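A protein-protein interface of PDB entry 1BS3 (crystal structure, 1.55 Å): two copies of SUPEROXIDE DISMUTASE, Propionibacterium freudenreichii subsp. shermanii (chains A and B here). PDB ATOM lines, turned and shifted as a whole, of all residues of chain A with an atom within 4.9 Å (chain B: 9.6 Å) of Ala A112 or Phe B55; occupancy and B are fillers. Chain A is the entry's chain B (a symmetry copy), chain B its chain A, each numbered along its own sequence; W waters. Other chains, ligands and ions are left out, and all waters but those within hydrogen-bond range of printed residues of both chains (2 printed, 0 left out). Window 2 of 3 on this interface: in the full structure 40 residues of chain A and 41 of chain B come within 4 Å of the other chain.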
ATOM      1  N   ASP A 108       4.528 -37.410 -14.541  1.00  0.00           N
ATOM      2  CA  ASP A 108       4.568 -37.211 -13.095  1.00  0.00           C
ATOM      3  C   ASP A 108       4.413 -35.744 -12.715  1.00  0.00           C
ATOM      4  O   ASP A 108       3.696 -35.422 -11.772  1.00  0.00           O
ATOM      5  CB  ASP A 108       5.870 -37.758 -12.512  1.00  0.00           C
ATOM      6  CG  ASP A 108       5.918 -39.274 -12.507  1.00  0.00           C
ATOM      7  OD1 ASP A 108       4.953 -39.906 -12.026  1.00  0.00           O
ATOM      8  OD2 ASP A 108       6.932 -39.835 -12.973  1.00  0.00           O
ATOM      9  N   ASN A 109       5.090 -34.860 -13.445  1.00  0.00           N
ATOM     10  CA  ASN A 109       5.002 -33.425 -13.176  1.00  0.00           C
ATOM     11  C   ASN A 109       3.581 -32.933 -13.368  1.00  0.00           C
ATOM     12  O   ASN A 109       3.094 -32.102 -12.603  1.00  0.00           O
ATOM     13  CB  ASN A 109       5.936 -32.639 -14.094  1.00  0.00           C
ATOM     14  CG  ASN A 109       7.379 -32.668 -13.633  1.00  0.00           C
ATOM     15  OD1 ASN A 109       7.729 -33.343 -12.663  1.00  0.00           O
ATOM     16  ND2 ASN A 109       8.227 -31.915 -14.322  1.00  0.00           N
ATOM     17  N   MET A 110       2.920 -33.450 -14.399  1.00  0.00           N
ATOM     18  CA  MET A 110       1.543 -33.077 -14.692  1.00  0.00           C
ATOM     19  C   MET A 110       0.639 -33.539 -13.550  1.00  0.00           C
ATOM     20  O   MET A 110      -0.178 -32.764 -13.052  1.00  0.00           O
ATOM     21  CB  MET A 110       1.101 -33.699 -16.019  1.00  0.00           C
ATOM     22  CG  MET A 110      -0.308 -33.327 -16.454  1.00  0.00           C
ATOM     23  SD  MET A 110      -1.584 -34.306 -15.650  1.00  0.00           S
ATOM     24  CE  MET A 110      -1.412 -35.837 -16.533  1.00  0.00           C
ATOM     25  N   LYS A 111       0.810 -34.789 -13.121  1.00  0.00           N
ATOM     26  CA  LYS A 111       0.014 -35.341 -12.030  1.00  0.00           C
ATOM     27  C   LYS A 111       0.177 -34.525 -10.760  1.00  0.00           C
ATOM     28  O   LYS A 111      -0.794 -34.252 -10.065  1.00  0.00           O
ATOM     29  CB  LYS A 111       0.412 -36.784 -11.738  1.00  0.00           C
ATOM     30  CG  LYS A 111      -0.246 -37.811 -12.623  1.00  0.00           C
ATOM     31  CD  LYS A 111       0.009 -39.207 -12.076  1.00  0.00           C
ATOM     32  CE  LYS A 111      -0.391 -39.313 -10.611  1.00  0.00           C
ATOM     33  NZ  LYS A 111      -0.244 -40.698 -10.080  1.00  0.00           N
ATOM     34  N   ALA A 112       1.415 -34.138 -10.469  1.00  0.00           N
ATOM     35  CA  ALA A 112       1.719 -33.352  -9.280  1.00  0.00           C
ATOM     36  C   ALA A 112       1.027 -31.991  -9.315  1.00  0.00           C
ATOM     37  O   ALA A 112       0.434 -31.565  -8.326  1.00  0.00           O
ATOM     38  CB  ALA A 112       3.223 -33.178  -9.132  1.00  0.00           C
ATOM     39  N   GLN A 113       1.073 -31.330 -10.466  1.00  0.00           N
ATOM     40  CA  GLN A 113       0.447 -30.020 -10.610  1.00  0.00           C
ATOM     41  C   GLN A 113      -1.075 -30.112 -10.548  1.00  0.00           C
ATOM     42  O   GLN A 113      -1.724 -29.305  -9.888  1.00  0.00           O
ATOM     43  CB  GLN A 113       0.877 -29.362 -11.917  1.00  0.00           C
ATOM     44  CG  GLN A 113       0.431 -27.919 -12.038  1.00  0.00           C
ATOM     45  CD  GLN A 113       1.026 -27.223 -13.239  1.00  0.00           C
ATOM     46  OE1 GLN A 113       2.240 -27.247 -13.444  1.00  0.00           O
ATOM     47  NE2 GLN A 113       0.173 -26.614 -14.055  1.00  0.00           N
ATOM     48  N   PHE A 114      -1.628 -31.116 -11.224  1.00  0.00           N
ATOM     49  CA  PHE A 114      -3.070 -31.343 -11.263  1.00  0.00           C
ATOM     50  C   PHE A 114      -3.575 -31.688  -9.862  1.00  0.00           C
ATOM     51  O   PHE A 114      -4.612 -31.181  -9.429  1.00  0.00           O
ATOM     52  CB  PHE A 114      -3.384 -32.486 -12.243  1.00  0.00           C
ATOM     53  CG  PHE A 114      -4.849 -32.675 -12.531  1.00  0.00           C
ATOM     54  CD1 PHE A 114      -5.646 -33.453 -11.697  1.00  0.00           C
ATOM     55  CD2 PHE A 114      -5.426 -32.104 -13.660  1.00  0.00           C
ATOM     56  CE1 PHE A 114      -6.997 -33.661 -11.987  1.00  0.00           C
ATOM     57  CE2 PHE A 114      -6.775 -32.306 -13.958  1.00  0.00           C
ATOM     58  CZ  PHE A 114      -7.560 -33.085 -13.119  1.00  0.00           C
ATOM     59  N   THR A 115      -2.827 -32.532  -9.154  1.00  0.00           N
ATOM     60  CA  THR A 115      -3.197 -32.944  -7.801  1.00  0.00           C
ATOM     61  C   THR A 115      -3.174 -31.753  -6.846  1.00  0.00           C
ATOM     62  O   THR A 115      -4.092 -31.582  -6.046  1.00  0.00           O
ATOM     63  CB  THR A 115      -2.269 -34.055  -7.263  1.00  0.00           C
ATOM     64  OG1 THR A 115      -2.381 -35.217  -8.098  1.00  0.00           O
ATOM     65  CG2 THR A 115      -2.655 -34.434  -5.837  1.00  0.00           C
ATOM     66  N   ALA A 116      -2.140 -30.920  -6.957  1.00  0.00           N
ATOM     67  CA  ALA A 116      -2.017 -29.742  -6.105  1.00  0.00           C
ATOM     68  C   ALA A 116      -3.183 -28.789  -6.347  1.00  0.00           C
ATOM     69  O   ALA A 116      -3.743 -28.236  -5.404  1.00  0.00           O
ATOM     70  CB  ALA A 116      -0.691 -29.038  -6.355  1.00  0.00           C
ATOM     71  N   LYS B  45       6.072 -19.224 -13.605  1.00  0.00           N
ATOM     72  CA  LYS B  45       5.979 -19.563 -12.195  1.00  0.00           C
ATOM     73  C   LYS B  45       5.538 -21.012 -12.003  1.00  0.00           C
ATOM     74  O   LYS B  45       6.036 -21.705 -11.118  1.00  0.00           O
ATOM     75  CB  LYS B  45       5.008 -18.610 -11.493  1.00  0.00           C
ATOM     76  CG  LYS B  45       5.685 -17.567 -10.627  1.00  0.00           C
ATOM     77  CD  LYS B  45       6.728 -16.790 -11.393  1.00  0.00           C
ATOM     78  CE  LYS B  45       7.663 -16.053 -10.443  1.00  0.00           C
ATOM     79  NZ  LYS B  45       8.387 -16.994  -9.530  1.00  0.00           N
ATOM     80  N   LEU B  46       4.604 -21.464 -12.836  1.00  0.00           N
ATOM     81  CA  LEU B  46       4.117 -22.836 -12.761  1.00  0.00           C
ATOM     82  C   LEU B  46       5.210 -23.814 -13.175  1.00  0.00           C
ATOM     83  O   LEU B  46       5.312 -24.911 -12.627  1.00  0.00           O
ATOM     84  CB  LEU B  46       2.879 -23.014 -13.637  1.00  0.00           C
ATOM     85  CG  LEU B  46       1.613 -22.402 -13.035  1.00  0.00           C
ATOM     86  CD1 LEU B  46       0.517 -22.327 -14.084  1.00  0.00           C
ATOM     87  CD2 LEU B  46       1.169 -23.222 -11.830  1.00  0.00           C
ATOM     88  N   ALA B  47       6.038 -23.393 -14.128  1.00  0.00           N
ATOM     89  CA  ALA B  47       7.140 -24.215 -14.612  1.00  0.00           C
ATOM     90  C   ALA B  47       8.175 -24.380 -13.508  1.00  0.00           C
ATOM     91  O   ALA B  47       8.717 -25.464 -13.311  1.00  0.00           O
ATOM     92  CB  ALA B  47       7.773 -23.575 -15.844  1.00  0.00           C
ATOM     93  N   GLU B  48       8.429 -23.298 -12.779  1.00  0.00           N
ATOM     94  CA  GLU B  48       9.384 -23.307 -11.677  1.00  0.00           C
ATOM     95  C   GLU B  48       8.866 -24.199 -10.550  1.00  0.00           C
ATOM     96  O   GLU B  48       9.641 -24.888  -9.884  1.00  0.00           O
ATOM     97  CB  GLU B  48       9.610 -21.885 -11.159  1.00  0.00           C
ATOM     98  CG  GLU B  48      10.598 -21.800 -10.005  1.00  0.00           C
ATOM     99  CD  GLU B  48      10.747 -20.390  -9.454  1.00  0.00           C
ATOM    100  OE1 GLU B  48       9.718 -19.766  -9.105  1.00  0.00           O
ATOM    101  OE2 GLU B  48      11.897 -19.906  -9.369  1.00  0.00           O
ATOM    102  N   ALA B  49       7.548 -24.183 -10.354  1.00  0.00           N
ATOM    103  CA  ALA B  49       6.895 -24.992  -9.326  1.00  0.00           C
ATOM    104  C   ALA B  49       7.085 -26.481  -9.611  1.00  0.00           C
ATOM    105  O   ALA B  49       7.380 -27.258  -8.704  1.00  0.00           O
ATOM    106  CB  ALA B  49       5.410 -24.659  -9.261  1.00  0.00           C
ATOM    107  N   ARG B  50       6.918 -26.874 -10.870  1.00  0.00           N
ATOM    108  CA  ARG B  50       7.088 -28.270 -11.263  1.00  0.00           C
ATOM    109  C   ARG B  50       8.542 -28.696 -11.110  1.00  0.00           C
ATOM    110  O   ARG B  50       8.823 -29.802 -10.648  1.00  0.00           O
ATOM    111  CB  ARG B  50       6.631 -28.499 -12.706  1.00  0.00           C
ATOM    112  CG  ARG B  50       5.125 -28.418 -12.909  1.00  0.00           C
ATOM    113  CD  ARG B  50       4.732 -28.847 -14.321  1.00  0.00           C
ATOM    114  NE  ARG B  50       5.389 -28.055 -15.360  1.00  0.00           N
ATOM    115  CZ  ARG B  50       4.897 -26.935 -15.882  1.00  0.00           C
ATOM    116  NH1 ARG B  50       3.730 -26.453 -15.471  1.00  0.00           N
ATOM    117  NH2 ARG B  50       5.577 -26.288 -16.818  1.00  0.00           N
ATOM    118  N   ASP B  51       9.464 -27.812 -11.482  1.00  0.00           N
ATOM    119  CA  ASP B  51      10.893 -28.105 -11.386  1.00  0.00           C
ATOM    120  C   ASP B  51      11.336 -28.390  -9.960  1.00  0.00           C
ATOM    121  O   ASP B  51      12.073 -29.343  -9.714  1.00  0.00           O
ATOM    122  CB  ASP B  51      11.727 -26.941 -11.936  1.00  0.00           C
ATOM    123  CG  ASP B  51      11.690 -26.851 -13.446  1.00  0.00           C
ATOM    124  OD1 ASP B  51      11.332 -27.849 -14.109  1.00  0.00           O
ATOM    125  OD2 ASP B  51      12.035 -25.774 -13.973  1.00  0.00           O
ATOM    126  N   LYS B  52      10.888 -27.547  -9.033  1.00  0.00           N
ATOM    127  CA  LYS B  52      11.246 -27.670  -7.624  1.00  0.00           C
ATOM    128  C   LYS B  52      10.278 -28.519  -6.809  1.00  0.00           C
ATOM    129  O   LYS B  52      10.506 -28.746  -5.619  1.00  0.00           O
ATOM    130  CB  LYS B  52      11.346 -26.279  -6.992  1.00  0.00           C
ATOM    131  CG  LYS B  52      12.438 -25.397  -7.575  1.00  0.00           C
ATOM    132  CD  LYS B  52      12.373 -23.994  -6.979  1.00  0.00           C
ATOM    133  CE  LYS B  52      13.512 -23.113  -7.481  1.00  0.00           C
ATOM    134  NZ  LYS B  52      13.442 -21.729  -6.918  1.00  0.00           N
ATOM    135  N   ALA B  53       9.208 -28.987  -7.448  1.00  0.00           N
ATOM    136  CA  ALA B  53       8.189 -29.793  -6.782  1.00  0.00           C
ATOM    137  C   ALA B  53       7.621 -28.992  -5.610  1.00  0.00           C
ATOM    138  O   ALA B  53       7.385 -29.525  -4.522  1.00  0.00           O
ATOM    139  CB  ALA B  53       8.780 -31.127  -6.302  1.00  0.00           C
ATOM    140  N   ASP B  54       7.448 -27.692  -5.835  1.00  0.00           N
ATOM    141  CA  ASP B  54       6.923 -26.791  -4.825  1.00  0.00           C
ATOM    142  C   ASP B  54       5.655 -26.130  -5.354  1.00  0.00           C
ATOM    143  O   ASP B  54       5.711 -25.152  -6.103  1.00  0.00           O
ATOM    144  CB  ASP B  54       7.981 -25.739  -4.472  1.00  0.00           C
ATOM    145  CG  ASP B  54       7.482 -24.707  -3.478  1.00  0.00           C
ATOM    146  OD1 ASP B  54       6.501 -24.975  -2.751  1.00  0.00           O
ATOM    147  OD2 ASP B  54       8.082 -23.612  -3.428  1.00  0.00           O
ATOM    148  N   PHE B  55       4.513 -26.666  -4.941  1.00  0.00           N
ATOM    149  CA  PHE B  55       3.225 -26.149  -5.375  1.00  0.00           C
ATOM    150  C   PHE B  55       2.496 -25.352  -4.286  1.00  0.00           C
ATOM    151  O   PHE B  55       1.270 -25.238  -4.301  1.00  0.00           O
ATOM    152  CB  PHE B  55       2.357 -27.303  -5.876  1.00  0.00           C
ATOM    153  CG  PHE B  55       2.940 -28.024  -7.057  1.00  0.00           C
ATOM    154  CD1 PHE B  55       2.746 -27.546  -8.349  1.00  0.00           C
ATOM    155  CD2 PHE B  55       3.708 -29.173  -6.878  1.00  0.00           C
ATOM    156  CE1 PHE B  55       3.310 -28.197  -9.448  1.00  0.00           C
ATOM    157  CE2 PHE B  55       4.276 -29.830  -7.969  1.00  0.00           C
ATOM    158  CZ  PHE B  55       4.076 -29.340  -9.255  1.00  0.00           C
ATOM    159  N   GLY B  56       3.266 -24.759  -3.378  1.00  0.00           N
ATOM    160  CA  GLY B  56       2.684 -23.984  -2.295  1.00  0.00           C
ATOM    161  C   GLY B  56       1.788 -22.833  -2.725  1.00  0.00           C
ATOM    162  O   GLY B  56       0.774 -22.558  -2.081  1.00  0.00           O
ATOM    163  N   ALA B  57       2.144 -22.176  -3.827  1.00  0.00           N
ATOM    164  CA  ALA B  57       1.374 -21.042  -4.336  1.00  0.00           C
ATOM    165  C   ALA B  57       0.414 -21.404  -5.473  1.00  0.00           C
ATOM    166  O   ALA B  57      -0.085 -20.522  -6.161  1.00  0.00           O
ATOM    167  CB  ALA B  57       2.329 -19.944  -4.800  1.00  0.00           C
ATOM    168  N   ILE B  58       0.124 -22.692  -5.638  1.00  0.00           N
ATOM    169  CA  ILE B  58      -0.751 -23.143  -6.714  1.00  0.00           C
ATOM    170  C   ILE B  58      -2.070 -22.373  -6.844  1.00  0.00           C
ATOM    171  O   ILE B  58      -2.482 -22.039  -7.948  1.00  0.00           O
ATOM    172  CB  ILE B  58      -1.014 -24.676  -6.633  1.00  0.00           C
ATOM    173  CG1 ILE B  58      -1.630 -25.174  -7.939  1.00  0.00           C
ATOM    174  CG2 ILE B  58      -1.900 -25.019  -5.440  1.00  0.00           C
ATOM    175  CD1 ILE B  58      -0.728 -24.992  -9.141  1.00  0.00           C
ATOM    176  N   ASN B  59      -2.722 -22.072  -5.725  1.00  0.00           N
ATOM    177  CA  ASN B  59      -3.991 -21.338  -5.774  1.00  0.00           C
ATOM    178  C   ASN B  59      -3.807 -19.942  -6.360  1.00  0.00           C
ATOM    179  O   ASN B  59      -4.655 -19.459  -7.113  1.00  0.00           O
ATOM    180  CB  ASN B  59      -4.621 -21.222  -4.385  1.00  0.00           C
ATOM    181  CG  ASN B  59      -5.086 -22.556  -3.839  1.00  0.00           C
ATOM    182  OD1 ASN B  59      -5.126 -23.559  -4.553  1.00  0.00           O
ATOM    183  ND2 ASN B  59      -5.458 -22.570  -2.564  1.00  0.00           N
ATOM    184  N   LYS B  60      -2.699 -19.303  -5.999  1.00  0.00           N
ATOM    185  CA  LYS B  60      -2.390 -17.967  -6.489  1.00  0.00           C
ATOM    186  C   LYS B  60      -2.084 -18.027  -7.982  1.00  0.00           C
ATOM    187  O   LYS B  60      -2.662 -17.281  -8.775  1.00  0.00           O
ATOM    188  CB  LYS B  60      -1.182 -17.391  -5.734  1.00  0.00           C
ATOM    189  CG  LYS B  60      -0.703 -16.027  -6.241  1.00  0.00           C
ATOM    190  CD  LYS B  60       0.608 -15.618  -5.572  1.00  0.00           C
ATOM    191  CE  LYS B  60       1.168 -14.325  -6.159  1.00  0.00           C
ATOM    192  NZ  LYS B  60       1.439 -14.442  -7.617  1.00  0.00           N
ATOM    193  N   LEU B  61      -1.206 -18.954  -8.352  1.00  0.00           N
ATOM    194  CA  LEU B  61      -0.785 -19.119  -9.736  1.00  0.00           C
ATOM    195  C   LEU B  61      -1.914 -19.479 -10.695  1.00  0.00           C
ATOM    196  O   LEU B  61      -1.935 -19.004 -11.828  1.00  0.00           O
ATOM    197  CB  LEU B  61       0.358 -20.133  -9.825  1.00  0.00           C
ATOM    198  CG  LEU B  61       1.557 -19.793  -8.933  1.00  0.00           C
ATOM    199  CD1 LEU B  61       2.677 -20.802  -9.135  1.00  0.00           C
ATOM    200  CD2 LEU B  61       2.045 -18.390  -9.244  1.00  0.00           C
ATOM    201  N   GLU B  62      -2.861 -20.295 -10.240  1.00  0.00           N
ATOM    202  CA  GLU B  62      -3.986 -20.685 -11.086  1.00  0.00           C
ATOM    203  C   GLU B  62      -4.952 -19.520 -11.304  1.00  0.00           C
ATOM    204  O   GLU B  62      -5.585 -19.422 -12.356  1.00  0.00           O
ATOM    205  CB  GLU B  62      -4.722 -21.893 -10.497  1.00  0.00           C
ATOM    206  CG  GLU B  62      -3.941 -23.202 -10.586  1.00  0.00           C
ATOM    207  CD  GLU B  62      -3.916 -23.814 -11.985  1.00  0.00           C
ATOM    208  OE1 GLU B  62      -4.092 -23.097 -12.993  1.00  0.00           O
ATOM    209  OE2 GLU B  62      -3.717 -25.039 -12.074  1.00  0.00           O
HETATM  210  O   HOH W   1       6.622 -31.638 -10.076  1.00  0.00           O
HETATM  211  O   HOH W   2       1.439 -24.903 -16.809  1.00  0.00           O
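Among the printed residues, pairs that only touch across the chains: Ala A116 with Phe B55, Gln A113 with Phe B55, Ala A112 with Phe B55, Ala A116 with Ile B58, Gln A113 with Leu B46 and Asn A109 with Arg B50.
No residue of chain B comes within 4 Å of Thr A115. Of the printed residues of chain A, Arg B50 touches Asn A109 (3.99 Å) and Gln A113 (2.6 Å). Printed residues of chain B within 4 Å of Gln A113: Leu B46 (3.9 Å), Arg B50 (2.6 Å) and Phe B55 (3.6 Å). Lys B45 touches none of the printed residues of chain A. Asp A108 touches none of the printed residues of chain B. The nearest printed residue of chain A that does not touch Arg B50 is Met A110 (4.9 Å).
No position is printed for both chains.
The guanidinium group (NH1) of Arg B50 lies within hydrogen-bond range of the side-chain amide oxygen (OE1) of Gln A113 (2.6 Å).
Water W1 lies within hydrogen-bond range of the backbone carbonyl oxygen of Arg B50 and the side-chain amide oxygen of Asn A109. Water W2 lies within hydrogen-bond range of NH1 of Arg B50 (3.1 Å) and NE2 of Gln A113 (3.5 Å).
Hydrophobic or aromatic side chains of chain B within 4 Å of the printed part of chain A: Phe B55 and Ile B58. Of the 9 printed residues of chain A, 4 touch a printed residue of chain B. Printed residues of chain A that touch a printed residue of chain B: Asn A109, Ala A112, Gln A113 and Ala A116. Hydrophobic or aromatic side chains of chain A that line the printed part of chain B: Ala A112 and Ala A116. Among the printed residues, no Asp or Glu carboxylate lies within 4 Å of a Lys or Arg side-chain nitrogen of the other chain.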
